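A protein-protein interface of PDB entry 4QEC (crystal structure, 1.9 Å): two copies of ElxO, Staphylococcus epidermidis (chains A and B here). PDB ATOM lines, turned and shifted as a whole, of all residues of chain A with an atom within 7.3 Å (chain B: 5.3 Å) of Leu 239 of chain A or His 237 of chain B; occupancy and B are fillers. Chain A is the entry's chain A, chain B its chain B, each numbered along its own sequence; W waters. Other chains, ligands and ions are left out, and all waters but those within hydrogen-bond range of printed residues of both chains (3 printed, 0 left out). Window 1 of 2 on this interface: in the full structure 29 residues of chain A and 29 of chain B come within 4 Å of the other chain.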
ATOM      1  N   LEU A 143       2.818   7.748 -18.117  1.00  0.00           N
ATOM      2  CA  LEU A 143       3.116   9.058 -18.738  1.00  0.00           C
ATOM      3  C   LEU A 143       2.843   9.080 -20.248  1.00  0.00           C
ATOM      4  O   LEU A 143       3.103  10.089 -20.930  1.00  0.00           O
ATOM      5  CB  LEU A 143       4.575   9.469 -18.465  1.00  0.00           C
ATOM      6  CG  LEU A 143       4.912   9.990 -17.052  1.00  0.00           C
ATOM      7  CD1 LEU A 143       6.414  10.061 -16.792  1.00  0.00           C
ATOM      8  CD2 LEU A 143       4.292  11.354 -16.789  1.00  0.00           C
ATOM      9  N   ASN A 178       8.616  10.976  -4.417  1.00  0.00           N
ATOM     10  CA  ASN A 178       8.910  10.937  -5.843  1.00  0.00           C
ATOM     11  C   ASN A 178       8.489   9.595  -6.412  1.00  0.00           C
ATOM     12  O   ASN A 178       8.070   8.698  -5.668  1.00  0.00           O
ATOM     13  CB  ASN A 178      10.405  11.175  -6.088  1.00  0.00           C
ATOM     14  CG  ASN A 178      10.874  12.525  -5.574  1.00  0.00           C
ATOM     15  OD1 ASN A 178      11.475  12.617  -4.498  1.00  0.00           O
ATOM     16  ND2 ASN A 178      10.637  13.569  -6.347  1.00  0.00           N
ATOM     17  N   ALA A 179       8.595   9.452  -7.729  1.00  0.00           N
ATOM     18  CA  ALA A 179       8.301   8.181  -8.373  1.00  0.00           C
ATOM     19  C   ALA A 179       9.361   7.871  -9.420  1.00  0.00           C
ATOM     20  O   ALA A 179      10.055   8.772  -9.906  1.00  0.00           O
ATOM     21  CB  ALA A 179       6.908   8.223  -9.012  1.00  0.00           C
ATOM     22  N   VAL A 180       9.502   6.595  -9.758  1.00  0.00           N
ATOM     23  CA  VAL A 180      10.279   6.226 -10.933  1.00  0.00           C
ATOM     24  C   VAL A 180       9.310   5.702 -11.989  1.00  0.00           C
ATOM     25  O   VAL A 180       8.266   5.154 -11.647  1.00  0.00           O
ATOM     26  CB  VAL A 180      11.400   5.199 -10.631  1.00  0.00           C
ATOM     27  CG1 VAL A 180      12.474   5.828  -9.743  1.00  0.00           C
ATOM     28  CG2 VAL A 180      10.836   3.927  -9.991  1.00  0.00           C
ATOM     29  N   ALA A 181       9.649   5.915 -13.256  1.00  0.00           N
ATOM     30  CA  ALA A 181       8.831   5.475 -14.390  1.00  0.00           C
ATOM     31  C   ALA A 181       9.700   4.556 -15.255  1.00  0.00           C
ATOM     32  O   ALA A 181      10.333   5.016 -16.193  1.00  0.00           O
ATOM     33  CB  ALA A 181       8.364   6.679 -15.194  1.00  0.00           C
ATOM     34  N   PRO A 182       9.776   3.258 -14.909  1.00  0.00           N
ATOM     35  CA  PRO A 182      10.662   2.392 -15.692  1.00  0.00           C
ATOM     36  C   PRO A 182      10.093   2.046 -17.064  1.00  0.00           C
ATOM     37  O   PRO A 182       8.875   1.970 -17.228  1.00  0.00           O
ATOM     38  CB  PRO A 182      10.773   1.121 -14.831  1.00  0.00           C
ATOM     39  CG  PRO A 182      10.342   1.538 -13.462  1.00  0.00           C
ATOM     40  CD  PRO A 182       9.261   2.565 -13.719  1.00  0.00           C
ATOM     41  N   ASP A 218      19.233  -0.790 -12.792  1.00  0.00           N
ATOM     42  CA  ASP A 218      18.913   0.563 -13.275  1.00  0.00           C
ATOM     43  C   ASP A 218      17.828   1.181 -12.388  1.00  0.00           C
ATOM     44  O   ASP A 218      17.948   2.322 -11.945  1.00  0.00           O
ATOM     45  CB  ASP A 218      18.393   0.548 -14.719  1.00  0.00           C
ATOM     46  CG  ASP A 218      19.448   0.129 -15.739  1.00  0.00           C
ATOM     47  OD1 ASP A 218      20.631   0.513 -15.608  1.00  0.00           O
ATOM     48  OD2 ASP A 218      19.073  -0.568 -16.702  1.00  0.00           O
ATOM     49  N   VAL A 219      16.775   0.414 -12.127  1.00  0.00           N
ATOM     50  CA  VAL A 219      15.643   0.923 -11.345  1.00  0.00           C
ATOM     51  C   VAL A 219      16.036   1.147  -9.878  1.00  0.00           C
ATOM     52  O   VAL A 219      15.719   2.185  -9.292  1.00  0.00           O
ATOM     53  CB  VAL A 219      14.402   0.016 -11.458  1.00  0.00           C
ATOM     54  CG1 VAL A 219      13.196   0.671 -10.785  1.00  0.00           C
ATOM     55  CG2 VAL A 219      14.088  -0.281 -12.927  1.00  0.00           C
ATOM     56  N   LYS A 221      18.945   1.791  -8.592  1.00  0.00           N
ATOM     57  CA  LYS A 221      19.814   2.961  -8.494  1.00  0.00           C
ATOM     58  C   LYS A 221      19.036   4.278  -8.510  1.00  0.00           C
ATOM     59  O   LYS A 221      19.358   5.186  -7.747  1.00  0.00           O
ATOM     60  CB  LYS A 221      20.868   2.958  -9.606  1.00  0.00           C
ATOM     61  CG  LYS A 221      21.867   1.803  -9.511  1.00  0.00           C
ATOM     62  CD  LYS A 221      23.070   2.214  -8.700  1.00  0.00           C
ATOM     63  CE  LYS A 221      24.164   1.157  -8.693  1.00  0.00           C
ATOM     64  NZ  LYS A 221      25.071   1.606  -7.603  1.00  0.00           N
ATOM     65  N   GLY A 222      18.023   4.373  -9.379  1.00  0.00           N
ATOM     66  CA  GLY A 222      17.171   5.568  -9.430  1.00  0.00           C
ATOM     67  C   GLY A 222      16.381   5.729  -8.139  1.00  0.00           C
ATOM     68  O   GLY A 222      16.286   6.834  -7.582  1.00  0.00           O
ATOM     69  N   ILE A 223      15.811   4.625  -7.654  1.00  0.00           N
ATOM     70  CA  ILE A 223      15.072   4.649  -6.394  1.00  0.00           C
ATOM     71  C   ILE A 223      15.987   5.091  -5.251  1.00  0.00           C
ATOM     72  O   ILE A 223      15.625   5.981  -4.467  1.00  0.00           O
ATOM     73  CB  ILE A 223      14.407   3.282  -6.086  1.00  0.00           C
ATOM     74  CG1 ILE A 223      13.274   3.009  -7.089  1.00  0.00           C
ATOM     75  CG2 ILE A 223      13.849   3.245  -4.658  1.00  0.00           C
ATOM     76  CD1 ILE A 223      12.644   1.631  -6.957  1.00  0.00           C
ATOM     77  N   PHE A 225      18.734   6.854  -5.384  1.00  0.00           N
ATOM     78  CA  PHE A 225      19.057   8.270  -5.550  1.00  0.00           C
ATOM     79  C   PHE A 225      17.966   9.171  -4.975  1.00  0.00           C
ATOM     80  O   PHE A 225      18.265  10.149  -4.289  1.00  0.00           O
ATOM     81  CB  PHE A 225      19.326   8.627  -7.029  1.00  0.00           C
ATOM     82  CG  PHE A 225      19.369  10.108  -7.287  1.00  0.00           C
ATOM     83  CD1 PHE A 225      20.502  10.858  -6.951  1.00  0.00           C
ATOM     84  CD2 PHE A 225      18.277  10.765  -7.842  1.00  0.00           C
ATOM     85  CE1 PHE A 225      20.534  12.234  -7.158  1.00  0.00           C
ATOM     86  CE2 PHE A 225      18.307  12.138  -8.059  1.00  0.00           C
ATOM     87  CZ  PHE A 225      19.434  12.873  -7.725  1.00  0.00           C
ATOM     88  N   LEU A 226      16.704   8.848  -5.251  1.00  0.00           N
ATOM     89  CA  LEU A 226      15.588   9.682  -4.778  1.00  0.00           C
ATOM     90  C   LEU A 226      15.330   9.522  -3.274  1.00  0.00           C
ATOM     91  O   LEU A 226      14.730  10.397  -2.643  1.00  0.00           O
ATOM     92  CB  LEU A 226      14.304   9.389  -5.578  1.00  0.00           C
ATOM     93  CG  LEU A 226      14.347   9.688  -7.092  1.00  0.00           C
ATOM     94  CD1 LEU A 226      13.193   9.016  -7.823  1.00  0.00           C
ATOM     95  CD2 LEU A 226      14.345  11.185  -7.385  1.00  0.00           C
ATOM     96  N   ILE A 234      14.614  17.413  -4.073  1.00  0.00           N
ATOM     97  CA  ILE A 234      13.865  16.777  -5.164  1.00  0.00           C
ATOM     98  C   ILE A 234      12.602  16.162  -4.591  1.00  0.00           C
ATOM     99  O   ILE A 234      12.664  15.225  -3.791  1.00  0.00           O
ATOM    100  CB  ILE A 234      14.693  15.721  -5.943  1.00  0.00           C
ATOM    101  CG1 ILE A 234      15.887  16.394  -6.624  1.00  0.00           C
ATOM    102  CG2 ILE A 234      13.814  15.022  -6.983  1.00  0.00           C
ATOM    103  CD1 ILE A 234      16.974  15.445  -7.123  1.00  0.00           C
ATOM    104  N   HIS A 237       8.637  14.555  -8.195  1.00  0.00           N
ATOM    105  CA  HIS A 237       9.243  14.331  -9.509  1.00  0.00           C
ATOM    106  C   HIS A 237       9.107  12.869  -9.923  1.00  0.00           C
ATOM    107  O   HIS A 237       9.123  11.972  -9.076  1.00  0.00           O
ATOM    108  CB  HIS A 237      10.726  14.755  -9.511  1.00  0.00           C
ATOM    109  CG  HIS A 237      11.410  14.527 -10.827  1.00  0.00           C
ATOM    110  ND1 HIS A 237      11.156  15.301 -11.942  1.00  0.00           N
ATOM    111  CD2 HIS A 237      12.303  13.584 -11.218  1.00  0.00           C
ATOM    112  CE1 HIS A 237      11.875  14.853 -12.957  1.00  0.00           C
ATOM    113  NE2 HIS A 237      12.581  13.813 -12.545  1.00  0.00           N
ATOM    114  N   VAL A 238       8.969  12.643 -11.227  1.00  0.00           N
ATOM    115  CA  VAL A 238       8.917  11.297 -11.778  1.00  0.00           C
ATOM    116  C   VAL A 238      10.163  11.103 -12.619  1.00  0.00           C
ATOM    117  O   VAL A 238      10.323  11.730 -13.663  1.00  0.00           O
ATOM    118  CB  VAL A 238       7.677  11.086 -12.673  1.00  0.00           C
ATOM    119  CG1 VAL A 238       7.585   9.624 -13.089  1.00  0.00           C
ATOM    120  CG2 VAL A 238       6.409  11.507 -11.944  1.00  0.00           C
ATOM    121  N   LEU A 239      11.043  10.228 -12.154  1.00  0.00           N
ATOM    122  CA  LEU A 239      12.306   9.982 -12.825  1.00  0.00           C
ATOM    123  C   LEU A 239      12.129   8.871 -13.852  1.00  0.00           C
ATOM    124  O   LEU A 239      11.865   7.736 -13.477  1.00  0.00           O
ATOM    125  CB  LEU A 239      13.350   9.565 -11.779  1.00  0.00           C
ATOM    126  CG  LEU A 239      14.737   9.141 -12.285  1.00  0.00           C
ATOM    127  CD1 LEU A 239      15.459  10.297 -12.975  1.00  0.00           C
ATOM    128  CD2 LEU A 239      15.554   8.598 -11.126  1.00  0.00           C
ATOM    129  N   SER A 240      12.294   9.182 -15.139  1.00  0.00           N
ATOM    130  CA  SER A 240      12.167   8.157 -16.189  1.00  0.00           C
ATOM    131  C   SER A 240      13.421   7.285 -16.226  1.00  0.00           C
ATOM    132  O   SER A 240      14.530   7.803 -16.227  1.00  0.00           O
ATOM    133  CB  SER A 240      11.974   8.803 -17.558  1.00  0.00           C
ATOM    134  OG  SER A 240      10.946   9.765 -17.514  1.00  0.00           O
ATOM    135  N   ILE A 241      13.236   5.969 -16.235  1.00  0.00           N
ATOM    136  CA  ILE A 241      14.358   5.024 -16.332  1.00  0.00           C
ATOM    137  C   ILE A 241      13.986   4.115 -17.496  1.00  0.00           C
ATOM    138  O   ILE A 241      13.510   2.996 -17.319  1.00  0.00           O
ATOM    139  CB  ILE A 241      14.602   4.276 -14.998  1.00  0.00           C
ATOM    140  CG1 ILE A 241      14.707   5.289 -13.835  1.00  0.00           C
ATOM    141  CG2 ILE A 241      15.884   3.445 -15.085  1.00  0.00           C
ATOM    142  CD1 ILE A 241      14.918   4.695 -12.452  1.00  0.00           C
ATOM    143  N   ASP A 242      14.158   4.639 -18.704  1.00  0.00           N
ATOM    144  CA  ASP A 242      13.420   4.105 -19.855  1.00  0.00           C
ATOM    145  C   ASP A 242      14.180   4.057 -21.170  1.00  0.00           C
ATOM    146  O   ASP A 242      13.561   3.937 -22.242  1.00  0.00           O
ATOM    147  CB  ASP A 242      12.134   4.913 -20.052  1.00  0.00           C
ATOM    148  CG  ASP A 242      12.391   6.359 -20.502  1.00  0.00           C
ATOM    149  OD1 ASP A 242      13.566   6.803 -20.581  1.00  0.00           O
ATOM    150  OD2 ASP A 242      11.393   7.065 -20.766  1.00  0.00           O
ATOM    151  N   GLY A 244      15.377   6.307 -22.871  1.00  0.00           N
ATOM    152  CA  GLY A 244      14.991   7.418 -23.746  1.00  0.00           C
ATOM    153  C   GLY A 244      13.554   7.383 -24.251  1.00  0.00           C
ATOM    154  O   GLY A 244      13.150   8.258 -25.016  1.00  0.00           O
ATOM    155  N   LEU A 246      10.477   8.095 -23.203  1.00  0.00           N
ATOM    156  CA  LEU A 246       9.562   9.231 -23.024  1.00  0.00           C
ATOM    157  C   LEU A 246      10.069  10.545 -23.648  1.00  0.00           C
ATOM    158  O   LEU A 246       9.312  11.505 -23.754  1.00  0.00           O
ATOM    159  CB  LEU A 246       9.203   9.424 -21.539  1.00  0.00           C
ATOM    160  CG  LEU A 246       8.356   8.302 -20.902  1.00  0.00           C
ATOM    161  CD1 LEU A 246       8.319   8.450 -19.384  1.00  0.00           C
ATOM    162  CD2 LEU A 246       6.941   8.263 -21.465  1.00  0.00           C
ATOM    163  N   SER A 247      11.330  10.569 -24.082  1.00  0.00           N
ATOM    164  CA  SER A 247      11.903  11.755 -24.723  1.00  0.00           C
ATOM    165  C   SER A 247      11.578  11.852 -26.217  1.00  0.00           C
ATOM    166  O   SER A 247      11.799  12.897 -26.832  1.00  0.00           O
ATOM    167  CB  SER A 247      13.410  11.792 -24.527  1.00  0.00           C
ATOM    168  OG  SER A 247      14.023  10.757 -25.278  1.00  0.00           O
ATOM    169  N   THR B 163      18.715  18.857 -25.595  1.00  0.00           N
ATOM    170  CA  THR B 163      18.893  17.674 -24.738  1.00  0.00           C
ATOM    171  C   THR B 163      18.111  16.456 -25.255  1.00  0.00           C
ATOM    172  O   THR B 163      18.679  15.372 -25.463  1.00  0.00           O
ATOM    173  CB  THR B 163      18.480  17.987 -23.275  1.00  0.00           C
ATOM    174  OG1 THR B 163      19.239  19.102 -22.806  1.00  0.00           O
ATOM    175  CG2 THR B 163      18.733  16.800 -22.348  1.00  0.00           C
ATOM    176  N   ILE B 177      22.409  11.589 -22.495  1.00  0.00           N
ATOM    177  CA  ILE B 177      22.313  13.031 -22.608  1.00  0.00           C
ATOM    178  C   ILE B 177      21.062  13.464 -21.860  1.00  0.00           C
ATOM    179  O   ILE B 177      19.936  13.155 -22.265  1.00  0.00           O
ATOM    180  CB  ILE B 177      22.252  13.486 -24.079  1.00  0.00           C
ATOM    181  CG1 ILE B 177      23.485  12.983 -24.859  1.00  0.00           C
ATOM    182  CG2 ILE B 177      22.136  15.001 -24.154  1.00  0.00           C
ATOM    183  CD1 ILE B 177      23.448  13.260 -26.348  1.00  0.00           C
ATOM    184  N   ASN B 178      21.271  14.172 -20.765  1.00  0.00           N
ATOM    185  CA  ASN B 178      20.169  14.565 -19.883  1.00  0.00           C
ATOM    186  C   ASN B 178      20.325  16.009 -19.461  1.00  0.00           C
ATOM    187  O   ASN B 178      21.314  16.654 -19.806  1.00  0.00           O
ATOM    188  CB  ASN B 178      20.139  13.679 -18.629  1.00  0.00           C
ATOM    189  CG  ASN B 178      19.857  12.218 -18.943  1.00  0.00           C
ATOM    190  OD1 ASN B 178      18.713  11.822 -19.133  1.00  0.00           O
ATOM    191  ND2 ASN B 178      20.903  11.403 -18.947  1.00  0.00           N
ATOM    192  N   ALA B 179      19.336  16.523 -18.730  1.00  0.00           N
ATOM    193  CA  ALA B 179      19.419  17.885 -18.200  1.00  0.00           C
ATOM    194  C   ALA B 179      18.920  17.940 -16.770  1.00  0.00           C
ATOM    195  O   ALA B 179      18.192  17.046 -16.316  1.00  0.00           O
ATOM    196  CB  ALA B 179      18.613  18.843 -19.068  1.00  0.00           C
ATOM    197  N   PHE B 225      24.679  12.199 -10.473  1.00  0.00           N
ATOM    198  CA  PHE B 225      23.840  11.015 -10.679  1.00  0.00           C
ATOM    199  C   PHE B 225      23.600  10.728 -12.160  1.00  0.00           C
ATOM    200  O   PHE B 225      23.673   9.580 -12.581  1.00  0.00           O
ATOM    201  CB  PHE B 225      22.490  11.142  -9.951  1.00  0.00           C
ATOM    202  CG  PHE B 225      21.482  10.081 -10.344  1.00  0.00           C
ATOM    203  CD1 PHE B 225      21.614   8.768  -9.886  1.00  0.00           C
ATOM    204  CD2 PHE B 225      20.421  10.388 -11.189  1.00  0.00           C
ATOM    205  CE1 PHE B 225      20.702   7.791 -10.259  1.00  0.00           C
ATOM    206  CE2 PHE B 225      19.497   9.409 -11.561  1.00  0.00           C
ATOM    207  CZ  PHE B 225      19.646   8.108 -11.098  1.00  0.00           C
ATOM    208  N   LEU B 226      23.305  11.768 -12.944  1.00  0.00           N
ATOM    209  CA  LEU B 226      22.992  11.570 -14.356  1.00  0.00           C
ATOM    210  C   LEU B 226      24.230  11.260 -15.189  1.00  0.00           C
ATOM    211  O   LEU B 226      24.118  10.646 -16.253  1.00  0.00           O
ATOM    212  CB  LEU B 226      22.262  12.787 -14.936  1.00  0.00           C
ATOM    213  CG  LEU B 226      20.855  13.047 -14.381  1.00  0.00           C
ATOM    214  CD1 LEU B 226      20.407  14.454 -14.735  1.00  0.00           C
ATOM    215  CD2 LEU B 226      19.868  12.024 -14.929  1.00  0.00           C
ATOM    216  N   ILE B 234      19.254   5.917 -18.291  1.00  0.00           N
ATOM    217  CA  ILE B 234      18.559   7.197 -18.224  1.00  0.00           C
ATOM    218  C   ILE B 234      19.103   8.128 -19.298  1.00  0.00           C
ATOM    219  O   ILE B 234      20.262   8.560 -19.246  1.00  0.00           O
ATOM    220  CB  ILE B 234      18.631   7.859 -16.822  1.00  0.00           C
ATOM    221  CG1 ILE B 234      18.007   6.932 -15.768  1.00  0.00           C
ATOM    222  CG2 ILE B 234      17.947   9.228 -16.846  1.00  0.00           C
ATOM    223  CD1 ILE B 234      18.280   7.328 -14.321  1.00  0.00           C
ATOM    224  N   THR B 235      18.261   8.425 -20.279  1.00  0.00           N
ATOM    225  CA  THR B 235      18.625   9.414 -21.287  1.00  0.00           C
ATOM    226  C   THR B 235      17.405  10.197 -21.767  1.00  0.00           C
ATOM    227  O   THR B 235      16.276   9.693 -21.724  1.00  0.00           O
ATOM    228  CB  THR B 235      19.467   8.798 -22.437  1.00  0.00           C
ATOM    229  OG1 THR B 235      20.123   9.843 -23.154  1.00  0.00           O
ATOM    230  CG2 THR B 235      18.600   7.949 -23.402  1.00  0.00           C
ATOM    231  N   GLY B 236      17.641  11.435 -22.204  1.00  0.00           N
ATOM    232  CA  GLY B 236      16.580  12.319 -22.688  1.00  0.00           C
ATOM    233  C   GLY B 236      15.697  12.869 -21.580  1.00  0.00           C
ATOM    234  O   GLY B 236      14.609  13.371 -21.849  1.00  0.00           O
ATOM    235  N   HIS B 237      16.176  12.800 -20.344  1.00  0.00           N
ATOM    236  CA  HIS B 237      15.359  13.143 -19.192  1.00  0.00           C
ATOM    237  C   HIS B 237      15.763  14.483 -18.595  1.00  0.00           C
ATOM    238  O   HIS B 237      16.951  14.843 -18.601  1.00  0.00           O
ATOM    239  CB  HIS B 237      15.460  12.058 -18.117  1.00  0.00           C
ATOM    240  CG  HIS B 237      14.595  12.325 -16.923  1.00  0.00           C
ATOM    241  ND1 HIS B 237      13.218  12.310 -16.986  1.00  0.00           N
ATOM    242  CD2 HIS B 237      14.910  12.648 -15.647  1.00  0.00           C
ATOM    243  CE1 HIS B 237      12.719  12.597 -15.797  1.00  0.00           C
ATOM    244  NE2 HIS B 237      13.726  12.800 -14.964  1.00  0.00           N
ATOM    245  N   VAL B 238      14.771  15.204 -18.072  1.00  0.00           N
ATOM    246  CA  VAL B 238      15.018  16.455 -17.378  1.00  0.00           C
ATOM    247  C   VAL B 238      14.682  16.239 -15.912  1.00  0.00           C
ATOM    248  O   VAL B 238      13.508  16.088 -15.548  1.00  0.00           O
ATOM    249  CB  VAL B 238      14.156  17.615 -17.927  1.00  0.00           C
ATOM    250  CG1 VAL B 238      14.568  18.926 -17.261  1.00  0.00           C
ATOM    251  CG2 VAL B 238      14.287  17.722 -19.441  1.00  0.00           C
ATOM    252  N   LEU B 239      15.723  16.219 -15.084  1.00  0.00           N
ATOM    253  CA  LEU B 239      15.586  16.016 -13.648  1.00  0.00           C
ATOM    254  C   LEU B 239      15.309  17.345 -12.937  1.00  0.00           C
ATOM    255  O   LEU B 239      16.178  18.204 -12.888  1.00  0.00           O
ATOM    256  CB  LEU B 239      16.871  15.376 -13.081  1.00  0.00           C
ATOM    257  CG  LEU B 239      16.980  15.154 -11.557  1.00  0.00           C
ATOM    258  CD1 LEU B 239      15.855  14.267 -11.016  1.00  0.00           C
ATOM    259  CD2 LEU B 239      18.354  14.588 -11.208  1.00  0.00           C
HETATM  260  O   HOH W   1      13.491   9.545 -21.442  1.00  0.00           O
HETATM  261  O   HOH W   2      12.029  11.297 -19.732  1.00  0.00           O
HETATM  262  O   HOH W   3      15.411   7.994 -18.954  1.00  0.00           O
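A ring nitrogen (NE2) of His 237 of chain B sits at hydrogen-bond distance from a ring nitrogen (NE2) of His 237 of chain A, 2.9 Å away.
A ring nitrogen (ND1) of His 237 of chain B is in hydrogen-bond range of the side-chain hydroxyl (OG) of Ser 240 of chain A, at 3.5 Å.
Water W3 lies within hydrogen-bond range of OD1 of Asp 242 of chain A (2.7 Å), O of Ser 240 of chain A (2.9 Å) and N of Thr 235 of chain B (3.2 Å).
Water W1 lies within hydrogen-bond range of O of Thr 235 of chain B (2.8 Å) and OD1 of Asp 242 of chain A (2.9 Å).
Water W2 bridges the side-chain hydroxyl (OG) of Ser 240 of chain A (2.9 Å) and a ring nitrogen (ND1) of His 237 of chain B (3.2 Å).
O of Lys 221 of chain A touches CE1 of Phe 225 of chain B (3.9 Å).
CA of Gly 222 of chain A touches CZ of Phe 225 of chain B (3.9 Å).
Phe 225 of chain A touches Phe 225 of chain B.
CE2 of Phe 225 of chain A touches CD2 of Leu 239 of chain B (3.99 Å).
His 237 of chain A touches Leu 239 of chain B (CD2 to CD1, 3.6 Å).
Val 238 of chain A touches His 237 of chain B.
Leu 239 of chain A touches His 237 of chain B.
Ser 240 of chain A touches Ile 234 of chain B.
Gly 244 of chain A touches Thr 235 of chain B.
Gly 236 of chain B touches Ser 247 of chain A (O to CB, 3.3 Å).
Printed residues of chain B within 4 Å of Phe 225 of chain A: Phe 225 (3.6 Å) and Leu 239 (3.99 Å).
Printed residues of chain B within 4 Å of Leu 239 of chain A: His 237 (3.6 Å).
Asp 242 of chain A touches none of the printed residues of chain B.
Printed residues of chain B within 4 Å of Gly 244 of chain A: Thr 235.
Of the printed residues of chain B, Ser 247 of chain A touches Gly 236.
Of the printed residues of chain A, Ile 234 of chain B touches Ser 240 (3.6 Å).
Gly 236 of chain B touches just one residue of chain A: Ser 247 (3.3 Å).
His 237 of chain B touches just these residues of chain A: His 237, Val 238, Leu 239 and Ser 240.
The nearest residue of chain B that does not touch Leu 239 of chain A is Phe 225 of chain B (4.05 Å).
The nearest printed residue of chain B that does not touch Ser 240 of chain A is Thr 235 of chain B (5.5 Å).
The backbone carbonyl oxygen (O) of His 237 of chain A sits at hydrogen-bond distance from the backbone NH (N) of Ala 179 of chain A, 2.9 Å away.
The side-chain carboxylate of Asp 242 of chain A is in hydrogen-bond range of the backbone NH of Gly 244 of chain A, at 3.0 Å.
The side-chain amide oxygen (OD1) of Asn 178 of chain B is in hydrogen-bond range of the backbone NH (N) of Gly 236 of chain B (3.3 Å).
The side-chain amide oxygen of Asn 178 of chain B is in hydrogen-bond range of the backbone NH of His 237 of chain B.
N of Ala 179 of chain B lies within hydrogen-bond range of O of His 237 of chain B.
O of Ala 179 of chain B is in hydrogen-bond range of N of Leu 239 of chain B (2.9 Å).
Of the 12 printed residues of chain B, 7 touch a printed residue of chain A.
Hydrophobic or aromatic side chains of chain B that line the printed part of chain A: Phe 225, Ile 234, His 237 and Leu 239.
Of the 23 printed residues of chain A, 9 touch a printed residue of chain B.
Printed residues of chain A that touch a printed residue of chain B: Lys 221, Gly 222, Phe 225, His 237, Val 238, Leu 239, Ser 240, Gly 244 and Ser 247.
Among the printed residues, 13 pairs touch across the chains.
Among the printed residues, no Asp or Glu carboxylate lies within 4 Å of a Lys or Arg side-chain nitrogen of the other chain.
Phe 225 of chain B touches its own counterpart, Phe 225 of chain A.
Phe 225 of chain A touches Leu 239 of chain B, but with the chains exchanged Leu 239 of chain A does not touch Phe 225 of chain B (4.05 Å).
His 237 of chain B touches its own counterpart, His 237 of chain A.
His 237 of chain A touches Val 238 of chain B, and with the chains exchanged Val 238 of chain A touches His 237 of chain B.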
